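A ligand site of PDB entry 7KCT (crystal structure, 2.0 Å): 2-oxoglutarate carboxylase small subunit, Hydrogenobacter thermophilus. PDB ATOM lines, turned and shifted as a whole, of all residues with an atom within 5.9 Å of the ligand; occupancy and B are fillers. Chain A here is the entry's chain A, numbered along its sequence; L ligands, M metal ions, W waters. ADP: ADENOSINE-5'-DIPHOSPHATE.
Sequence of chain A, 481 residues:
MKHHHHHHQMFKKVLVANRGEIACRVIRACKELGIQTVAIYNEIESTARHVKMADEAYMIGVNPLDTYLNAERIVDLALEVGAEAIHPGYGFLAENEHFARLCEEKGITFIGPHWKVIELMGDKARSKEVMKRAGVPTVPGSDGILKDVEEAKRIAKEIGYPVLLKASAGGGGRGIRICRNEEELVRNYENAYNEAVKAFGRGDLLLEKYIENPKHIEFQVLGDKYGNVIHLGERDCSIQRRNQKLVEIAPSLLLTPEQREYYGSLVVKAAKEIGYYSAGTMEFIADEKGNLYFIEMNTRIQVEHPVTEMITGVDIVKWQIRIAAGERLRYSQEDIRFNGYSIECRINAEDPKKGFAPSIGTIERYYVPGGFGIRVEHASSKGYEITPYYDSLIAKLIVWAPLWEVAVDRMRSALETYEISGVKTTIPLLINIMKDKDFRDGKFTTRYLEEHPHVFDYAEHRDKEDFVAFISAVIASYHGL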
ATOM      1  N   TYR A  90       8.713 -10.048 -20.945  1.00  0.00           N
ATOM      2  CA  TYR A  90       7.654 -10.330 -19.984  1.00  0.00           C
ATOM      3  C   TYR A  90       6.511  -9.341 -20.194  1.00  0.00           C
ATOM      4  O   TYR A  90       6.703  -8.277 -20.769  1.00  0.00           O
ATOM      5  CB  TYR A  90       8.192 -10.290 -18.514  1.00  0.00           C
ATOM      6  CG  TYR A  90       8.918  -9.040 -18.060  1.00  0.00           C
ATOM      7  CD1 TYR A  90       8.249  -7.822 -17.970  1.00  0.00           C
ATOM      8  CD2 TYR A  90      10.268  -9.081 -17.711  1.00  0.00           C
ATOM      9  CE1 TYR A  90       8.899  -6.680 -17.538  1.00  0.00           C
ATOM     10  CE2 TYR A  90      10.930  -7.941 -17.292  1.00  0.00           C
ATOM     11  CZ  TYR A  90      10.240  -6.742 -17.235  1.00  0.00           C
ATOM     12  OH  TYR A  90      10.840  -5.590 -16.807  1.00  0.00           O
ATOM     13  N   GLY A  91       5.287  -9.731 -19.802  1.00  0.00           N
ATOM     14  CA  GLY A  91       4.148  -8.886 -20.127  1.00  0.00           C
ATOM     15  C   GLY A  91       3.829  -8.928 -21.616  1.00  0.00           C
ATOM     16  O   GLY A  91       4.339  -9.741 -22.384  1.00  0.00           O
ATOM     17  N   PHE A  92       2.985  -7.966 -22.025  1.00  0.00           N
ATOM     18  CA  PHE A  92       2.572  -7.854 -23.424  1.00  0.00           C
ATOM     19  C   PHE A  92       2.164  -9.227 -23.962  1.00  0.00           C
ATOM     20  O   PHE A  92       1.189  -9.771 -23.467  1.00  0.00           O
ATOM     21  CB  PHE A  92       3.686  -7.204 -24.224  1.00  0.00           C
ATOM     22  CG  PHE A  92       3.986  -5.768 -23.793  1.00  0.00           C
ATOM     23  CD1 PHE A  92       2.963  -4.842 -23.677  1.00  0.00           C
ATOM     24  CD2 PHE A  92       5.272  -5.359 -23.520  1.00  0.00           C
ATOM     25  CE1 PHE A  92       3.224  -3.521 -23.304  1.00  0.00           C
ATOM     26  CE2 PHE A  92       5.541  -4.059 -23.117  1.00  0.00           C
ATOM     27  CZ  PHE A  92       4.517  -3.128 -23.045  1.00  0.00           C
ATOM     28  N   GLU A  95       2.896 -14.382 -22.645  1.00  0.00           N
ATOM     29  CA  GLU A  95       2.077 -15.526 -22.259  1.00  0.00           C
ATOM     30  C   GLU A  95       0.796 -15.589 -23.098  1.00  0.00           C
ATOM     31  O   GLU A  95      -0.238 -16.073 -22.635  1.00  0.00           O
ATOM     32  CB  GLU A  95       1.756 -15.470 -20.775  1.00  0.00           C
ATOM     33  CG  GLU A  95       2.974 -15.570 -19.899  1.00  0.00           C
ATOM     34  N   ALA A 169      -8.122 -15.846 -15.188  1.00  0.00           N
ATOM     35  CA  ALA A 169      -7.343 -15.311 -16.304  1.00  0.00           C
ATOM     36  C   ALA A 169      -6.384 -14.191 -15.895  1.00  0.00           C
ATOM     37  O   ALA A 169      -6.127 -13.278 -16.689  1.00  0.00           O
ATOM     38  CB  ALA A 169      -8.290 -14.813 -17.412  1.00  0.00           C
ATOM     39  N   GLY A 170      -5.831 -14.274 -14.675  1.00  0.00           N
ATOM     40  CA  GLY A 170      -5.227 -13.137 -14.015  1.00  0.00           C
ATOM     41  C   GLY A 170      -3.721 -13.005 -14.209  1.00  0.00           C
ATOM     42  O   GLY A 170      -3.036 -13.943 -14.607  1.00  0.00           O
ATOM     43  N   GLY A 171      -3.259 -11.787 -13.951  1.00  0.00           N
ATOM     44  CA  GLY A 171      -1.849 -11.446 -13.945  1.00  0.00           C
ATOM     45  C   GLY A 171      -1.665 -10.085 -13.326  1.00  0.00           C
ATOM     46  O   GLY A 171      -2.635  -9.323 -13.171  1.00  0.00           O
ATOM     47  N   GLY A 172      -0.425  -9.785 -12.959  1.00  0.00           N
ATOM     48  CA  GLY A 172      -0.055  -8.490 -12.420  1.00  0.00           C
ATOM     49  C   GLY A 172      -0.895  -7.952 -11.280  1.00  0.00           C
ATOM     50  O   GLY A 172      -0.955  -6.739 -11.061  1.00  0.00           O
ATOM     51  N   PHE A 200      -9.030  -8.561 -18.431  1.00  0.00           N
ATOM     52  CA  PHE A 200      -8.440  -9.740 -19.050  1.00  0.00           C
ATOM     53  C   PHE A 200      -9.302 -10.325 -20.163  1.00  0.00           C
ATOM     54  O   PHE A 200      -8.862 -11.279 -20.823  1.00  0.00           O
ATOM     55  CB  PHE A 200      -8.155 -10.839 -18.000  1.00  0.00           C
ATOM     56  CG  PHE A 200      -7.351 -10.372 -16.798  1.00  0.00           C
ATOM     57  CD1 PHE A 200      -6.011 -10.029 -16.930  1.00  0.00           C
ATOM     58  CD2 PHE A 200      -7.933 -10.293 -15.542  1.00  0.00           C
ATOM     59  CE1 PHE A 200      -5.258  -9.609 -15.828  1.00  0.00           C
ATOM     60  CE2 PHE A 200      -7.193  -9.877 -14.436  1.00  0.00           C
ATOM     61  CZ  PHE A 200      -5.849  -9.533 -14.581  1.00  0.00           C
ATOM     62  N   GLU A 218       8.799 -18.540  -4.703  1.00  0.00           N
ATOM     63  CA  GLU A 218       8.645 -18.978  -6.091  1.00  0.00           C
ATOM     64  C   GLU A 218       9.892 -19.678  -6.566  1.00  0.00           C
ATOM     65  O   GLU A 218      11.008 -19.318  -6.173  1.00  0.00           O
ATOM     66  CB  GLU A 218       8.292 -17.784  -7.006  1.00  0.00           C
ATOM     67  CG  GLU A 218       9.408 -16.803  -7.107  1.00  0.00           C
ATOM     68  CD  GLU A 218       9.037 -15.613  -7.939  1.00  0.00           C
ATOM     69  OE1 GLU A 218       7.827 -15.415  -8.170  1.00  0.00           O
ATOM     70  OE2 GLU A 218       9.963 -14.854  -8.346  1.00  0.00           O
ATOM     71  N   GLN A 244       1.746  -6.743  -6.261  1.00  0.00           N
ATOM     72  CA  GLN A 244       2.860  -6.758  -7.205  1.00  0.00           C
ATOM     73  C   GLN A 244       4.165  -6.495  -6.465  1.00  0.00           C
ATOM     74  O   GLN A 244       4.243  -5.675  -5.550  1.00  0.00           O
ATOM     75  CB  GLN A 244       2.635  -5.720  -8.290  1.00  0.00           C
ATOM     76  CG  GLN A 244       3.408  -5.928  -9.549  1.00  0.00           C
ATOM     77  CD  GLN A 244       3.194  -4.766 -10.515  1.00  0.00           C
ATOM     78  OE1 GLN A 244       2.141  -4.091 -10.478  1.00  0.00           O
ATOM     79  NE2 GLN A 244       4.181  -4.510 -11.371  1.00  0.00           N
ATOM     80  N   LYS A 245       5.206  -7.208  -6.899  1.00  0.00           N
ATOM     81  CA  LYS A 245       6.433  -7.276  -6.128  1.00  0.00           C
ATOM     82  C   LYS A 245       7.213  -5.972  -6.189  1.00  0.00           C
ATOM     83  O   LYS A 245       7.136  -5.208  -7.141  1.00  0.00           O
ATOM     84  CB  LYS A 245       7.275  -8.439  -6.628  1.00  0.00           C
ATOM     85  CG  LYS A 245       6.491  -9.756  -6.569  1.00  0.00           C
ATOM     86  CD  LYS A 245       7.014 -10.778  -7.556  1.00  0.00           C
ATOM     87  CE  LYS A 245       6.057 -11.955  -7.685  1.00  0.00           C
ATOM     88  NZ  LYS A 245       6.285 -12.658  -8.970  1.00  0.00           N
ATOM     89  N   GLU A 248      12.717  -8.406  -3.909  1.00  0.00           N
ATOM     90  CA  GLU A 248      12.876  -9.836  -4.090  1.00  0.00           C
ATOM     91  C   GLU A 248      14.238 -10.294  -3.609  1.00  0.00           C
ATOM     92  O   GLU A 248      15.244  -9.612  -3.843  1.00  0.00           O
ATOM     93  CB  GLU A 248      12.684 -10.171  -5.597  1.00  0.00           C
ATOM     94  CG  GLU A 248      11.367  -9.677  -6.189  1.00  0.00           C
ATOM     95  CD  GLU A 248      11.500  -8.434  -7.085  1.00  0.00           C
ATOM     96  OE1 GLU A 248      12.597  -7.826  -7.203  1.00  0.00           O
ATOM     97  OE2 GLU A 248      10.486  -8.097  -7.745  1.00  0.00           O
ATOM     98  N   GLU A 283       4.777 -20.338  -8.650  1.00  0.00           N
ATOM     99  CA  GLU A 283       4.644 -19.487  -7.481  1.00  0.00           C
ATOM    100  C   GLU A 283       3.841 -20.241  -6.418  1.00  0.00           C
ATOM    101  O   GLU A 283       2.830 -20.888  -6.755  1.00  0.00           O
ATOM    102  CB  GLU A 283       3.971 -18.167  -7.849  1.00  0.00           C
ATOM    103  CG  GLU A 283       4.715 -17.408  -8.989  1.00  0.00           C
ATOM    104  CD  GLU A 283       4.250 -15.957  -9.197  1.00  0.00           C
ATOM    105  OE1 GLU A 283       5.117 -15.100  -9.459  1.00  0.00           O
ATOM    106  OE2 GLU A 283       3.024 -15.665  -9.181  1.00  0.00           O
ATOM    107  N   ASN A 298       4.068 -18.970 -14.046  1.00  0.00           N
ATOM    108  CA  ASN A 298       4.281 -17.927 -15.045  1.00  0.00           C
ATOM    109  C   ASN A 298       5.148 -18.571 -16.126  1.00  0.00           C
ATOM    110  O   ASN A 298       6.268 -18.994 -15.832  1.00  0.00           O
ATOM    111  CB  ASN A 298       4.990 -16.687 -14.465  1.00  0.00           C
ATOM    112  CG  ASN A 298       4.077 -15.813 -13.620  1.00  0.00           C
ATOM    113  OD1 ASN A 298       4.528 -15.170 -12.671  1.00  0.00           O
ATOM    114  ND2 ASN A 298       2.821 -15.708 -14.004  1.00  0.00           N
ATOM    115  N   ARG A 300       7.125 -17.824 -18.598  1.00  0.00           N
ATOM    116  CA  ARG A 300       7.919 -16.738 -19.182  1.00  0.00           C
ATOM    117  C   ARG A 300       9.024 -16.388 -18.197  1.00  0.00           C
ATOM    118  O   ARG A 300       9.034 -16.833 -17.047  1.00  0.00           O
ATOM    119  CB  ARG A 300       7.043 -15.537 -19.498  1.00  0.00           C
ATOM    120  CG  ARG A 300       6.175 -15.044 -18.294  1.00  0.00           C
ATOM    121  CD  ARG A 300       5.803 -13.571 -18.387  1.00  0.00           C
ATOM    122  NE  ARG A 300       4.965 -13.082 -17.286  1.00  0.00           N
ATOM    123  CZ  ARG A 300       5.422 -12.610 -16.122  1.00  0.00           C
ATOM    124  NH1 ARG A 300       6.737 -12.554 -15.861  1.00  0.00           N
ATOM    125  NH2 ARG A 300       4.540 -12.166 -15.213  1.00  0.00           N
ATOM    126  N   ILE A 301       9.969 -15.575 -18.662  1.00  0.00           N
ATOM    127  CA  ILE A 301      10.929 -14.945 -17.751  1.00  0.00           C
ATOM    128  C   ILE A 301      10.161 -13.990 -16.842  1.00  0.00           C
ATOM    129  O   ILE A 301       9.126 -13.440 -17.234  1.00  0.00           O
ATOM    130  CB  ILE A 301      12.019 -14.206 -18.544  1.00  0.00           C
ATOM    131  CG1 ILE A 301      13.245 -13.942 -17.669  1.00  0.00           C
ATOM    132  CG2 ILE A 301      11.473 -12.892 -19.139  1.00  0.00           C
ATOM    133  CD1 ILE A 301      14.119 -15.150 -17.412  1.00  0.00           C
ATOM    134  N   GLN A 302      10.652 -13.798 -15.634  1.00  0.00           N
ATOM    135  CA  GLN A 302      10.097 -12.792 -14.734  1.00  0.00           C
ATOM    136  C   GLN A 302      11.071 -11.633 -14.501  1.00  0.00           C
ATOM    137  O   GLN A 302      12.291 -11.789 -14.577  1.00  0.00           O
ATOM    138  CB  GLN A 302       9.779 -13.417 -13.381  1.00  0.00           C
ATOM    139  CG  GLN A 302       8.742 -14.484 -13.398  1.00  0.00           C
ATOM    140  CD  GLN A 302       8.434 -14.961 -11.998  1.00  0.00           C
ATOM    141  OE1 GLN A 302       9.321 -15.462 -11.309  1.00  0.00           O
ATOM    142  NE2 GLN A 302       7.215 -14.747 -11.543  1.00  0.00           N
ATOM    143  N   VAL A 303      10.505 -10.497 -14.082  1.00  0.00           N
ATOM    144  CA  VAL A 303      11.286  -9.310 -13.751  1.00  0.00           C
ATOM    145  C   VAL A 303      12.479  -9.628 -12.864  1.00  0.00           C
ATOM    146  O   VAL A 303      13.600  -9.182 -13.123  1.00  0.00           O
ATOM    147  CB  VAL A 303      10.338  -8.284 -13.064  1.00  0.00           C
ATOM    148  CG1 VAL A 303      11.110  -7.110 -12.424  1.00  0.00           C
ATOM    149  CG2 VAL A 303       9.333  -7.749 -14.080  1.00  0.00           C
ATOM    150  N   GLU A 304      12.263 -10.454 -11.847  1.00  0.00           N
ATOM    151  CA  GLU A 304      13.217 -10.673 -10.773  1.00  0.00           C
ATOM    152  C   GLU A 304      14.187 -11.826 -11.021  1.00  0.00           C
ATOM    153  O   GLU A 304      14.906 -12.237 -10.080  1.00  0.00           O
ATOM    154  CB  GLU A 304      12.426 -10.884  -9.454  1.00  0.00           C
ATOM    155  CG  GLU A 304      11.472 -12.132  -9.449  1.00  0.00           C
ATOM    156  CD  GLU A 304       9.998 -11.875  -9.885  1.00  0.00           C
ATOM    157  OE1 GLU A 304       9.679 -10.898 -10.587  1.00  0.00           O
ATOM    158  OE2 GLU A 304       9.104 -12.673  -9.488  1.00  0.00           O
ATOM    159  N   ARG A 346      12.951  -2.870  -7.033  1.00  0.00           N
ATOM    160  CA  ARG A 346      12.370  -2.222  -8.207  1.00  0.00           C
ATOM    161  C   ARG A 346      12.341  -0.741  -7.938  1.00  0.00           C
ATOM    162  O   ARG A 346      11.748  -0.288  -6.946  1.00  0.00           O
ATOM    163  CB  ARG A 346      10.961  -2.740  -8.483  1.00  0.00           C
ATOM    164  CG  ARG A 346      10.946  -4.233  -8.597  1.00  0.00           C
ATOM    165  CD  ARG A 346       9.765  -4.658  -9.384  1.00  0.00           C
ATOM    166  NE  ARG A 346       9.622  -6.104  -9.420  1.00  0.00           N
ATOM    167  CZ  ARG A 346       8.672  -6.706 -10.110  1.00  0.00           C
ATOM    168  NH1 ARG A 346       7.836  -5.942 -10.811  1.00  0.00           N
ATOM    169  NH2 ARG A 346       8.538  -8.028 -10.080  1.00  0.00           N
ATOM    170  N   ASP A 391       4.412   0.416 -17.866  1.00  0.00           N
ATOM    171  CA  ASP A 391       4.815   0.175 -16.491  1.00  0.00           C
ATOM    172  C   ASP A 391       5.744   1.293 -15.987  1.00  0.00           C
ATOM    173  O   ASP A 391       6.460   1.963 -16.754  1.00  0.00           O
ATOM    174  CB  ASP A 391       5.488  -1.208 -16.343  1.00  0.00           C
HETATM  175  PB  ADP L   1       6.790 -10.642 -12.562  1.00  0.00           P
HETATM  176  O1B ADP L   1       7.699 -10.798 -13.760  1.00  0.00           O
HETATM  177  O2B ADP L   1       7.217 -11.093 -11.185  1.00  0.00           O
HETATM  178  O3B ADP L   1       5.328 -10.814 -12.830  1.00  0.00           O
HETATM  179  PA  ADP L   1       5.371  -8.082 -12.514  1.00  0.00           P
HETATM  180  O1A ADP L   1       5.390  -6.588 -12.530  1.00  0.00           O
HETATM  181  O2A ADP L   1       4.151  -8.899 -12.136  1.00  0.00           O
HETATM  182  O3A ADP L   1       6.712  -8.842 -12.133  1.00  0.00           O
HETATM  183  O5' ADP L   1       5.195  -8.338 -14.461  1.00  0.00           O
HETATM  184  C5' ADP L   1       5.728  -7.168 -15.219  1.00  0.00           C
HETATM  185  C4' ADP L   1       4.866  -6.723 -16.304  1.00  0.00           C
HETATM  186  O4' ADP L   1       4.017  -7.703 -16.863  1.00  0.00           O
HETATM  187  C3' ADP L   1       3.958  -5.583 -15.559  1.00  0.00           C
HETATM  188  O3' ADP L   1       3.760  -4.583 -16.408  1.00  0.00           O
HETATM  189  C2' ADP L   1       2.704  -6.502 -15.303  1.00  0.00           C
HETATM  190  O2' ADP L   1       1.543  -5.812 -15.345  1.00  0.00           O
HETATM  191  C1' ADP L   1       2.760  -7.274 -16.657  1.00  0.00           C
HETATM  192  N9  ADP L   1       2.089  -8.630 -16.641  1.00  0.00           N
HETATM  193  C8  ADP L   1       2.259  -9.710 -15.738  1.00  0.00           C
HETATM  194  N7  ADP L   1       1.476 -10.777 -16.012  1.00  0.00           N
HETATM  195  C5  ADP L   1       0.793 -10.406 -17.157  1.00  0.00           C
HETATM  196  C6  ADP L   1      -0.162 -11.094 -17.918  1.00  0.00           C
HETATM  197  N6  ADP L   1      -0.568 -12.368 -17.567  1.00  0.00           N
HETATM  198  N1  ADP L   1      -0.711 -10.508 -19.031  1.00  0.00           N
HETATM  199  C2  ADP L   1      -0.273  -9.211 -19.288  1.00  0.00           C
HETATM  200  N3  ADP L   1       0.630  -8.431 -18.649  1.00  0.00           N
HETATM  201  C4  ADP L   1       1.163  -9.082 -17.572  1.00  0.00           C
HETATM  202 MG    MG M   1       1.673 -14.011  -9.616  1.00  0.00          MG
HETATM  203  O   HOH W   1       3.860  -4.410 -19.171  1.00  0.00           O
HETATM  204  O   HOH W   2       4.514  -8.940  -9.239  1.00  0.00           O
HETATM  205  O   HOH W   3       1.793  -6.094 -20.273  1.00  0.00           O
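An oxygen (O2B) of the ligand lies close to the side-chain carboxylate (OE1) of Glu 304, at 2.5 Å. The side-chain amide nitrogen of Gln 244 is in hydrogen-bond range of an oxygen (O1A) of the ligand (2.7 Å). The backbone NH (N) of Val 303 lies within hydrogen-bond range of an oxygen (O1B) of the ligand. NH2 of Arg 300 is in salt-bridge range of O3B of the ligand, at 2.9 Å. The guanidinium group (NH1) of Arg 346 lies within salt-bridge range of an oxygen (O1A) of the ligand (3.1 Å). O2B of the ligand is in salt-bridge range of NZ of Lys 245, at 2.9 Å.
The side-chain amide oxygen (OE1) of Gln 302 sits close to the side-chain carboxylate (OE2) of Glu 304 (3.3 Å). NE of Arg 346 is in hydrogen-bond range of O of Lys 245, 3.5 Å away. The side-chain amino group (NZ) of Lys 245 sits close to the side-chain amide nitrogen (NE2) of Gln 302, at 3.4 Å. The side-chain amino group of Lys 245 is in salt-bridge range of the side-chain carboxylate of Glu 283, 2.8 Å away. The side-chain amino group of Lys 245 lies within salt-bridge range of the side-chain carboxylate of Glu 218. The side-chain amide oxygen (OD1) of Asn 298 lies within hydrogen-bond range of the side-chain amide nitrogen (NE2) of Gln 302, 2.9 Å away. The side-chain carboxylate (OE1) of Glu 283 is in hydrogen-bond range of the side-chain amide nitrogen (NE2) of Gln 302, 3.0 Å away. OE1 of Gln 302 lies close to OE2 of Glu 218, at 3.1 Å.
CD1 of Tyr 90 touches C5' of the ligand (3.8 Å). Gly 91 touches the ligand. Gly 171 touches the ligand. Gly 172 touches the ligand. Gln 302 touches the ligand. Asp 391 touches the ligand. Hydrophobic or aromatic side chains that line the ligand: Tyr 90 and Val 303.
Water W2 lies within hydrogen-bond range of O2A of the ligand (2.9 Å) and N of Lys 245 (3.0 Å). Water W3 lies within hydrogen-bond range of the backbone NH (N) of Phe 92 (2.8 Å) and a nitrogen (N3) of the ligand (3.1 Å).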
